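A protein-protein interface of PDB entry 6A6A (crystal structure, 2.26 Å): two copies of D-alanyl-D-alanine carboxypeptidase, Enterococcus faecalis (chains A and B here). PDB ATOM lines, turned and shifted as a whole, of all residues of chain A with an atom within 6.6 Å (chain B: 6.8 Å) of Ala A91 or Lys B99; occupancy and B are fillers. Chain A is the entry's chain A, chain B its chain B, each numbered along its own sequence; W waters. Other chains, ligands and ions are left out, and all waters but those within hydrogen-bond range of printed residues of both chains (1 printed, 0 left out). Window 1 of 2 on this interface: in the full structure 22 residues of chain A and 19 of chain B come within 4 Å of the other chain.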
ATOM      1  N   SER A  61      32.844  -1.153   5.800  1.00  0.00           N
ATOM      2  CA  SER A  61      33.019  -2.608   5.856  1.00  0.00           C
ATOM      3  C   SER A  61      31.713  -3.309   6.266  1.00  0.00           C
ATOM      4  O   SER A  61      31.424  -4.382   5.751  1.00  0.00           O
ATOM      5  CB  SER A  61      34.154  -2.970   6.760  1.00  0.00           C
ATOM      6  OG  SER A  61      34.001  -2.354   8.021  1.00  0.00           O
ATOM      7  N   ASN A  62      30.882  -2.657   7.100  1.00  0.00           N
ATOM      8  CA  ASN A  62      29.711  -3.324   7.682  1.00  0.00           C
ATOM      9  C   ASN A  62      28.524  -3.197   6.736  1.00  0.00           C
ATOM     10  O   ASN A  62      27.451  -3.695   7.046  1.00  0.00           O
ATOM     11  CB  ASN A  62      29.368  -2.822   9.083  1.00  0.00           C
ATOM     12  CG  ASN A  62      28.889  -1.393   9.143  1.00  0.00           C
ATOM     13  OD1 ASN A  62      28.971  -0.643   8.151  1.00  0.00           O
ATOM     14  ND2 ASN A  62      28.387  -1.018  10.313  1.00  0.00           N
ATOM     15  N   GLY A  63      28.732  -2.477   5.631  1.00  0.00           N
ATOM     16  CA  GLY A  63      27.722  -2.279   4.602  1.00  0.00           C
ATOM     17  C   GLY A  63      27.004  -0.947   4.737  1.00  0.00           C
ATOM     18  O   GLY A  63      26.453  -0.446   3.776  1.00  0.00           O
ATOM     19  N   GLU A  64      26.992  -0.367   5.941  1.00  0.00           N
ATOM     20  CA  GLU A  64      26.470   1.002   6.090  1.00  0.00           C
ATOM     21  C   GLU A  64      27.216   1.921   5.101  1.00  0.00           C
ATOM     22  O   GLU A  64      28.362   1.618   4.709  1.00  0.00           O
ATOM     23  CB  GLU A  64      26.641   1.499   7.529  1.00  0.00           C
ATOM     24  CG  GLU A  64      25.834   0.727   8.548  1.00  0.00           C
ATOM     25  CD  GLU A  64      24.341   0.664   8.271  1.00  0.00           C
ATOM     26  OE1 GLU A  64      23.789   1.686   7.841  1.00  0.00           O
ATOM     27  OE2 GLU A  64      23.740  -0.409   8.489  1.00  0.00           O
ATOM     28  N   ILE A  89      30.830   0.905  16.786  1.00  0.00           N
ATOM     29  CA  ILE A  89      30.336   0.469  15.496  1.00  0.00           C
ATOM     30  C   ILE A  89      29.459   1.573  14.908  1.00  0.00           C
ATOM     31  O   ILE A  89      28.837   2.371  15.624  1.00  0.00           O
ATOM     32  CB  ILE A  89      29.538  -0.841  15.624  1.00  0.00           C
ATOM     33  CG1 ILE A  89      28.361  -0.688  16.587  1.00  0.00           C
ATOM     34  CG2 ILE A  89      30.446  -2.016  16.006  1.00  0.00           C
ATOM     35  CD1 ILE A  89      27.113  -1.440  16.128  1.00  0.00           C
ATOM     36  N   VAL A  90      29.338   1.546  13.582  1.00  0.00           N
ATOM     37  CA  VAL A  90      28.299   2.290  12.935  1.00  0.00           C
ATOM     38  C   VAL A  90      27.079   1.364  12.807  1.00  0.00           C
ATOM     39  O   VAL A  90      27.035   0.507  11.946  1.00  0.00           O
ATOM     40  CB  VAL A  90      28.777   2.842  11.580  1.00  0.00           C
ATOM     41  CG1 VAL A  90      27.690   3.650  10.918  1.00  0.00           C
ATOM     42  CG2 VAL A  90      30.046   3.656  11.725  1.00  0.00           C
ATOM     43  N   ALA A  91      26.117   1.535  13.716  1.00  0.00           N
ATOM     44  CA  ALA A  91      24.813   0.888  13.649  1.00  0.00           C
ATOM     45  C   ALA A  91      24.058   1.365  12.402  1.00  0.00           C
ATOM     46  O   ALA A  91      23.572   0.571  11.611  1.00  0.00           O
ATOM     47  CB  ALA A  91      24.017   1.208  14.898  1.00  0.00           C
ATOM     48  N   SER A  92      23.964   2.685  12.233  1.00  0.00           N
ATOM     49  CA  SER A  92      23.185   3.244  11.138  1.00  0.00           C
ATOM     50  C   SER A  92      23.906   4.453  10.534  1.00  0.00           C
ATOM     51  O   SER A  92      24.327   5.353  11.253  1.00  0.00           O
ATOM     52  CB  SER A  92      21.794   3.610  11.624  1.00  0.00           C
ATOM     53  OG  SER A  92      20.994   4.055  10.547  1.00  0.00           O
ATOM     54  N   GLY A  93      23.991   4.459   9.203  1.00  0.00           N
ATOM     55  CA  GLY A  93      24.617   5.498   8.409  1.00  0.00           C
ATOM     56  C   GLY A  93      23.592   6.220   7.547  1.00  0.00           C
ATOM     57  O   GLY A  93      22.590   6.730   8.043  1.00  0.00           O
ATOM     58  N   ARG A  95      20.387   6.525   5.388  1.00  0.00           N
ATOM     59  CA  ARG A  95      19.107   5.817   5.245  1.00  0.00           C
ATOM     60  C   ARG A  95      18.307   6.497   4.135  1.00  0.00           C
ATOM     61  O   ARG A  95      18.275   7.726   4.076  1.00  0.00           O
ATOM     62  CB  ARG A  95      18.215   5.920   6.488  1.00  0.00           C
ATOM     63  CG  ARG A  95      18.786   5.365   7.781  1.00  0.00           C
ATOM     64  CD  ARG A  95      17.953   5.917   8.925  1.00  0.00           C
ATOM     65  NE  ARG A  95      18.389   5.381  10.202  1.00  0.00           N
ATOM     66  CZ  ARG A  95      18.417   6.053  11.339  1.00  0.00           C
ATOM     67  NH1 ARG A  95      17.587   7.070  11.538  1.00  0.00           N
ATOM     68  NH2 ARG A  95      19.290   5.689  12.265  1.00  0.00           N
ATOM     69  N   VAL A 143      25.818   9.432  11.732  1.00  0.00           N
ATOM     70  CA  VAL A 143      25.985   8.028  12.129  1.00  0.00           C
ATOM     71  C   VAL A 143      25.424   7.844  13.540  1.00  0.00           C
ATOM     72  O   VAL A 143      25.553   8.721  14.409  1.00  0.00           O
ATOM     73  CB  VAL A 143      27.444   7.536  12.031  1.00  0.00           C
ATOM     74  CG1 VAL A 143      27.890   7.396  10.587  1.00  0.00           C
ATOM     75  CG2 VAL A 143      28.406   8.411  12.808  1.00  0.00           C
ATOM     76  N   ASP A 144      24.783   6.687  13.714  1.00  0.00           N
ATOM     77  CA  ASP A 144      24.352   6.168  14.991  1.00  0.00           C
ATOM     78  C   ASP A 144      25.421   5.168  15.413  1.00  0.00           C
ATOM     79  O   ASP A 144      25.572   4.140  14.762  1.00  0.00           O
ATOM     80  CB  ASP A 144      23.000   5.467  14.870  1.00  0.00           C
ATOM     81  CG  ASP A 144      21.848   6.418  14.639  1.00  0.00           C
ATOM     82  OD1 ASP A 144      21.971   7.536  15.093  1.00  0.00           O
ATOM     83  OD2 ASP A 144      20.845   6.016  14.029  1.00  0.00           O
ATOM     84  N   ILE A 145      26.210   5.546  16.424  1.00  0.00           N
ATOM     85  CA  ILE A 145      27.286   4.763  16.888  1.00  0.00           C
ATOM     86  C   ILE A 145      26.857   4.010  18.163  1.00  0.00           C
ATOM     87  O   ILE A 145      26.263   4.566  19.087  1.00  0.00           O
ATOM     88  CB  ILE A 145      28.510   5.660  17.124  1.00  0.00           C
ATOM     89  CG1 ILE A 145      28.879   6.474  15.878  1.00  0.00           C
ATOM     90  CG2 ILE A 145      29.693   4.830  17.592  1.00  0.00           C
ATOM     91  CD1 ILE A 145      29.679   7.736  16.200  1.00  0.00           C
ATOM     92  N   ASN A 146      27.230   2.737  18.224  1.00  0.00           N
ATOM     93  CA  ASN A 146      26.967   1.877  19.351  1.00  0.00           C
ATOM     94  C   ASN A 146      28.291   1.178  19.689  1.00  0.00           C
ATOM     95  O   ASN A 146      29.263   1.264  18.932  1.00  0.00           O
ATOM     96  CB  ASN A 146      25.805   0.922  19.024  1.00  0.00           C
ATOM     97  CG  ASN A 146      24.450   1.608  18.976  1.00  0.00           C
ATOM     98  OD1 ASN A 146      24.253   2.659  19.575  1.00  0.00           O
ATOM     99  ND2 ASN A 146      23.499   1.037  18.258  1.00  0.00           N
ATOM    100  N   TRP A 189      23.648   7.830  20.777  1.00  0.00           N
ATOM    101  CA  TRP A 189      24.283   7.183  19.613  1.00  0.00           C
ATOM    102  C   TRP A 189      24.409   8.137  18.403  1.00  0.00           C
ATOM    103  O   TRP A 189      25.223   7.950  17.550  1.00  0.00           O
ATOM    104  CB  TRP A 189      23.487   5.930  19.223  1.00  0.00           C
ATOM    105  CG  TRP A 189      22.014   6.179  19.202  1.00  0.00           C
ATOM    106  CD1 TRP A 189      21.300   6.680  18.167  1.00  0.00           C
ATOM    107  CD2 TRP A 189      21.069   5.945  20.263  1.00  0.00           C
ATOM    108  NE1 TRP A 189      19.984   6.808  18.512  1.00  0.00           N
ATOM    109  CE2 TRP A 189      19.809   6.363  19.794  1.00  0.00           C
ATOM    110  CE3 TRP A 189      21.157   5.442  21.565  1.00  0.00           C
ATOM    111  CZ2 TRP A 189      18.654   6.287  20.573  1.00  0.00           C
ATOM    112  CZ3 TRP A 189      20.018   5.384  22.342  1.00  0.00           C
ATOM    113  CH2 TRP A 189      18.785   5.797  21.849  1.00  0.00           C
ATOM    114  N   SER B  92      16.254  -6.977   6.769  1.00  0.00           N
ATOM    115  CA  SER B  92      17.643  -7.355   6.548  1.00  0.00           C
ATOM    116  C   SER B  92      17.780  -8.299   5.355  1.00  0.00           C
ATOM    117  O   SER B  92      17.235  -9.413   5.395  1.00  0.00           O
ATOM    118  CB  SER B  92      18.222  -8.011   7.760  1.00  0.00           C
ATOM    119  OG  SER B  92      19.577  -8.365   7.555  1.00  0.00           O
ATOM    120  N   TYR B  94      21.208  -8.691   2.306  1.00  0.00           N
ATOM    121  CA  TYR B  94      22.635  -8.999   2.232  1.00  0.00           C
ATOM    122  C   TYR B  94      23.353  -8.391   3.450  1.00  0.00           C
ATOM    123  O   TYR B  94      23.038  -7.288   3.901  1.00  0.00           O
ATOM    124  CB  TYR B  94      23.283  -8.508   0.925  1.00  0.00           C
ATOM    125  CG  TYR B  94      24.783  -8.693   0.906  1.00  0.00           C
ATOM    126  CD1 TYR B  94      25.355  -9.923   0.628  1.00  0.00           C
ATOM    127  CD2 TYR B  94      25.630  -7.673   1.296  1.00  0.00           C
ATOM    128  CE1 TYR B  94      26.729 -10.114   0.683  1.00  0.00           C
ATOM    129  CE2 TYR B  94      27.003  -7.845   1.354  1.00  0.00           C
ATOM    130  CZ  TYR B  94      27.555  -9.071   1.057  1.00  0.00           C
ATOM    131  OH  TYR B  94      28.904  -9.241   1.121  1.00  0.00           O
ATOM    132  N   ARG B  95      24.334  -9.131   3.980  1.00  0.00           N
ATOM    133  CA  ARG B  95      25.218  -8.593   5.025  1.00  0.00           C
ATOM    134  C   ARG B  95      26.663  -8.946   4.728  1.00  0.00           C
ATOM    135  O   ARG B  95      26.952 -10.084   4.391  1.00  0.00           O
ATOM    136  CB  ARG B  95      24.939  -9.210   6.389  1.00  0.00           C
ATOM    137  CG  ARG B  95      23.594  -8.839   6.980  1.00  0.00           C
ATOM    138  CD  ARG B  95      23.467  -9.697   8.214  1.00  0.00           C
ATOM    139  NE  ARG B  95      22.136  -9.606   8.692  1.00  0.00           N
ATOM    140  CZ  ARG B  95      21.448 -10.607   9.184  1.00  0.00           C
ATOM    141  NH1 ARG B  95      22.058 -11.674   9.670  1.00  0.00           N
ATOM    142  NH2 ARG B  95      20.136 -10.515   9.159  1.00  0.00           N
ATOM    143  N   THR B  96      27.542  -7.972   4.950  1.00  0.00           N
ATOM    144  CA  THR B  96      28.965  -8.212   4.929  1.00  0.00           C
ATOM    145  C   THR B  96      29.330  -9.070   6.144  1.00  0.00           C
ATOM    146  O   THR B  96      28.596  -9.137   7.125  1.00  0.00           O
ATOM    147  CB  THR B  96      29.743  -6.888   4.870  1.00  0.00           C
ATOM    148  OG1 THR B  96      29.532  -6.169   6.084  1.00  0.00           O
ATOM    149  CG2 THR B  96      29.356  -6.011   3.697  1.00  0.00           C
ATOM    150  N   THR B  97      30.475  -9.742   6.040  1.00  0.00           N
ATOM    151  CA  THR B  97      31.157 -10.376   7.143  1.00  0.00           C
ATOM    152  C   THR B  97      31.161  -9.472   8.377  1.00  0.00           C
ATOM    153  O   THR B  97      30.876  -9.925   9.476  1.00  0.00           O
ATOM    154  CB  THR B  97      32.625 -10.640   6.793  1.00  0.00           C
ATOM    155  OG1 THR B  97      32.622 -11.438   5.613  1.00  0.00           O
ATOM    156  CG2 THR B  97      33.376 -11.336   7.907  1.00  0.00           C
ATOM    157  N   GLU B  98      31.494  -8.198   8.173  1.00  0.00           N
ATOM    158  CA  GLU B  98      31.663  -7.287   9.264  1.00  0.00           C
ATOM    159  C   GLU B  98      30.282  -6.988   9.853  1.00  0.00           C
ATOM    160  O   GLU B  98      30.145  -6.872  11.051  1.00  0.00           O
ATOM    161  CB  GLU B  98      32.402  -6.021   8.819  1.00  0.00           C
ATOM    162  CG  GLU B  98      32.500  -4.948   9.907  1.00  0.00           C
ATOM    163  CD  GLU B  98      33.113  -5.402  11.226  1.00  0.00           C
ATOM    164  OE1 GLU B  98      33.908  -6.336  11.202  1.00  0.00           O
ATOM    165  OE2 GLU B  98      32.786  -4.807  12.283  1.00  0.00           O
ATOM    166  N   LYS B  99      29.263  -6.874   9.001  1.00  0.00           N
ATOM    167  CA  LYS B  99      27.944  -6.593   9.487  1.00  0.00           C
ATOM    168  C   LYS B  99      27.488  -7.764  10.356  1.00  0.00           C
ATOM    169  O   LYS B  99      27.009  -7.559  11.469  1.00  0.00           O
ATOM    170  CB  LYS B  99      26.948  -6.380   8.350  1.00  0.00           C
ATOM    171  CG  LYS B  99      25.547  -5.989   8.809  1.00  0.00           C
ATOM    172  CD  LYS B  99      25.503  -4.871   9.847  1.00  0.00           C
ATOM    173  CE  LYS B  99      24.123  -4.246   9.962  1.00  0.00           C
ATOM    174  NZ  LYS B  99      24.180  -2.782  10.216  1.00  0.00           N
ATOM    175  N   GLN B 100      27.674  -8.979   9.828  1.00  0.00           N
ATOM    176  CA  GLN B 100      27.368 -10.202  10.535  1.00  0.00           C
ATOM    177  C   GLN B 100      28.102 -10.194  11.877  1.00  0.00           C
ATOM    178  O   GLN B 100      27.505 -10.459  12.903  1.00  0.00           O
ATOM    179  CB  GLN B 100      27.745 -11.421   9.705  1.00  0.00           C
ATOM    180  CG  GLN B 100      27.174 -12.709  10.261  1.00  0.00           C
ATOM    181  CD  GLN B 100      25.666 -12.752  10.175  1.00  0.00           C
ATOM    182  OE1 GLN B 100      25.055 -12.022   9.407  1.00  0.00           O
ATOM    183  NE2 GLN B 100      25.051 -13.614  10.969  1.00  0.00           N
ATOM    184  N   GLN B 101      29.395  -9.859  11.831  1.00  0.00           N
ATOM    185  CA  GLN B 101      30.239  -9.796  13.011  1.00  0.00           C
ATOM    186  C   GLN B 101      29.591  -8.899  14.069  1.00  0.00           C
ATOM    187  O   GLN B 101      29.609  -9.182  15.233  1.00  0.00           O
ATOM    188  CB  GLN B 101      31.626  -9.254  12.648  1.00  0.00           C
ATOM    189  CG  GLN B 101      32.645  -9.370  13.778  1.00  0.00           C
ATOM    190  CD  GLN B 101      32.899 -10.818  14.113  1.00  0.00           C
ATOM    191  OE1 GLN B 101      33.443 -11.570  13.307  1.00  0.00           O
ATOM    192  NE2 GLN B 101      32.463 -11.229  15.294  1.00  0.00           N
ATOM    193  N   GLU B 102      29.081  -7.754  13.635  1.00  0.00           N
ATOM    194  CA  GLU B 102      28.637  -6.722  14.575  1.00  0.00           C
ATOM    195  C   GLU B 102      27.349  -7.134  15.288  1.00  0.00           C
ATOM    196  O   GLU B 102      27.234  -6.881  16.450  1.00  0.00           O
ATOM    197  CB  GLU B 102      28.498  -5.400  13.838  1.00  0.00           C
ATOM    198  CG  GLU B 102      29.846  -4.766  13.665  1.00  0.00           C
ATOM    199  CD  GLU B 102      29.880  -3.586  12.718  1.00  0.00           C
ATOM    200  OE1 GLU B 102      28.813  -3.077  12.363  1.00  0.00           O
ATOM    201  OE2 GLU B 102      30.993  -3.206  12.339  1.00  0.00           O
ATOM    202  N   ILE B 103      26.433  -7.783  14.558  1.00  0.00           N
ATOM    203  CA  ILE B 103      25.202  -8.330  15.080  1.00  0.00           C
ATOM    204  C   ILE B 103      25.495  -9.382  16.155  1.00  0.00           C
ATOM    205  O   ILE B 103      24.923  -9.303  17.235  1.00  0.00           O
ATOM    206  CB  ILE B 103      24.376  -8.962  13.949  1.00  0.00           C
ATOM    207  CG1 ILE B 103      23.959  -7.923  12.919  1.00  0.00           C
ATOM    208  CG2 ILE B 103      23.191  -9.748  14.527  1.00  0.00           C
ATOM    209  CD1 ILE B 103      23.355  -8.536  11.668  1.00  0.00           C
ATOM    210  N   MET B 104      26.400 -10.301  15.816  1.00  0.00           N
ATOM    211  CA  MET B 104      26.865 -11.430  16.649  1.00  0.00           C
ATOM    212  C   MET B 104      27.521 -10.885  17.913  1.00  0.00           C
ATOM    213  O   MET B 104      27.147 -11.336  18.962  1.00  0.00           O
ATOM    214  CB  MET B 104      27.899 -12.235  15.862  1.00  0.00           C
ATOM    215  CG  MET B 104      28.496 -13.411  16.588  1.00  0.00           C
ATOM    216  SD  MET B 104      27.304 -14.619  17.174  1.00  0.00           S
ATOM    217  CE  MET B 104      28.400 -15.786  17.965  1.00  0.00           C
ATOM    218  N   GLU B 106      27.014  -7.919  19.171  1.00  0.00           N
ATOM    219  CA  GLU B 106      25.939  -7.284  19.961  1.00  0.00           C
ATOM    220  C   GLU B 106      25.114  -8.344  20.706  1.00  0.00           C
ATOM    221  O   GLU B 106      24.722  -8.090  21.823  1.00  0.00           O
ATOM    222  CB  GLU B 106      25.155  -6.246  19.165  1.00  0.00           C
ATOM    223  CG  GLU B 106      25.847  -4.901  19.179  1.00  0.00           C
ATOM    224  CD  GLU B 106      24.966  -3.706  18.904  1.00  0.00           C
ATOM    225  OE1 GLU B 106      25.004  -2.756  19.698  1.00  0.00           O
ATOM    226  OE2 GLU B 106      24.237  -3.742  17.912  1.00  0.00           O
ATOM    227  N   PRO B 132      30.065 -15.128  11.211  1.00  0.00           N
ATOM    228  CA  PRO B 132      30.447 -14.628   9.886  1.00  0.00           C
ATOM    229  C   PRO B 132      31.107 -15.763   9.082  1.00  0.00           C
ATOM    230  O   PRO B 132      31.855 -16.558   9.630  1.00  0.00           O
ATOM    231  CB  PRO B 132      31.424 -13.474  10.162  1.00  0.00           C
ATOM    232  CG  PRO B 132      31.128 -13.066  11.595  1.00  0.00           C
ATOM    233  CD  PRO B 132      30.618 -14.308  12.304  1.00  0.00           C
HETATM  234  O   HOH W   1      26.168  -5.192   5.590  1.00  0.00           O
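2 positions are printed for both chains. Of the 11 pairs that touch across the chains among the printed residues, none has its exchanged pair printed and touching as well.
The side-chain amide oxygen (OD1) of Asn A62 is in hydrogen-bond range of the backbone NH (N) of Glu A64 (3.0 Å). ND2 of Asn A62 is in hydrogen-bond range of O of Val A90 (2.6 Å). The side-chain carboxylate (OE1) of Glu A64 is in hydrogen-bond range of the backbone NH (N) of Gly A93, at 3.1 Å. The backbone NH (N) of Ala A91 lies within hydrogen-bond range of the backbone carbonyl oxygen (O) of Asp A144. The backbone NH (N) of Lys B99 is in hydrogen-bond range of the side-chain hydroxyl (OG1) of Thr B96 (3.0 Å). The side-chain carboxylate of Glu B102 lies close to the side-chain carboxylate of Glu B98 (2.4 Å).
Water W1 bridges O of Asn A62 and N of Thr B96.
Among the printed residues, 11 pairs touch across the chains. Among the printed residues, Asp or Glu carboxylates within 4 Å of a Lys or Arg side-chain nitrogen of the other chain: Glu A64 with Lys B99.
Of the printed residues of chain B, Gly A63 touches Thr B96 (3.8 Å). Printed residues of chain B within 4 Å of Ile A89: Glu B102 (3.7 Å). Of chain B, only Lys B99 comes within 4 Å of Ala A91. Printed residues of chain B within 4 Å of Asn A146: Glu B106 (3.8 Å). Of the printed residues of chain A, Glu B98 touches Ser A61 and Asn A62. Lys B99 touches three residues of chain A. The nearest printed residue of chain B that does not touch Glu A64 is Glu B102 (6.2 Å).
O of Ser A61 sits at hydrogen-bond distance from OG1 of Thr B96, 2.6 Å away. O of Asn A62 lies close to OG1 of Thr B96, at 3.4 Å. ND2 of Asn A62 is in hydrogen-bond range of OE1 of Glu B102. The side-chain amino group (NZ) of Lys B99 lies within salt-bridge range of the side-chain carboxylate (OE2) of Glu A64.
Among the printed residues, pairs that only touch across the chains: Ser A61 with Glu B98, Asn A62 with Glu B98, Asn A62 with Lys B99, Gly A63 with Thr B96, Ile A89 with Glu B102, Ala A91 with Lys B99 and Asn A146 with Glu B106.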
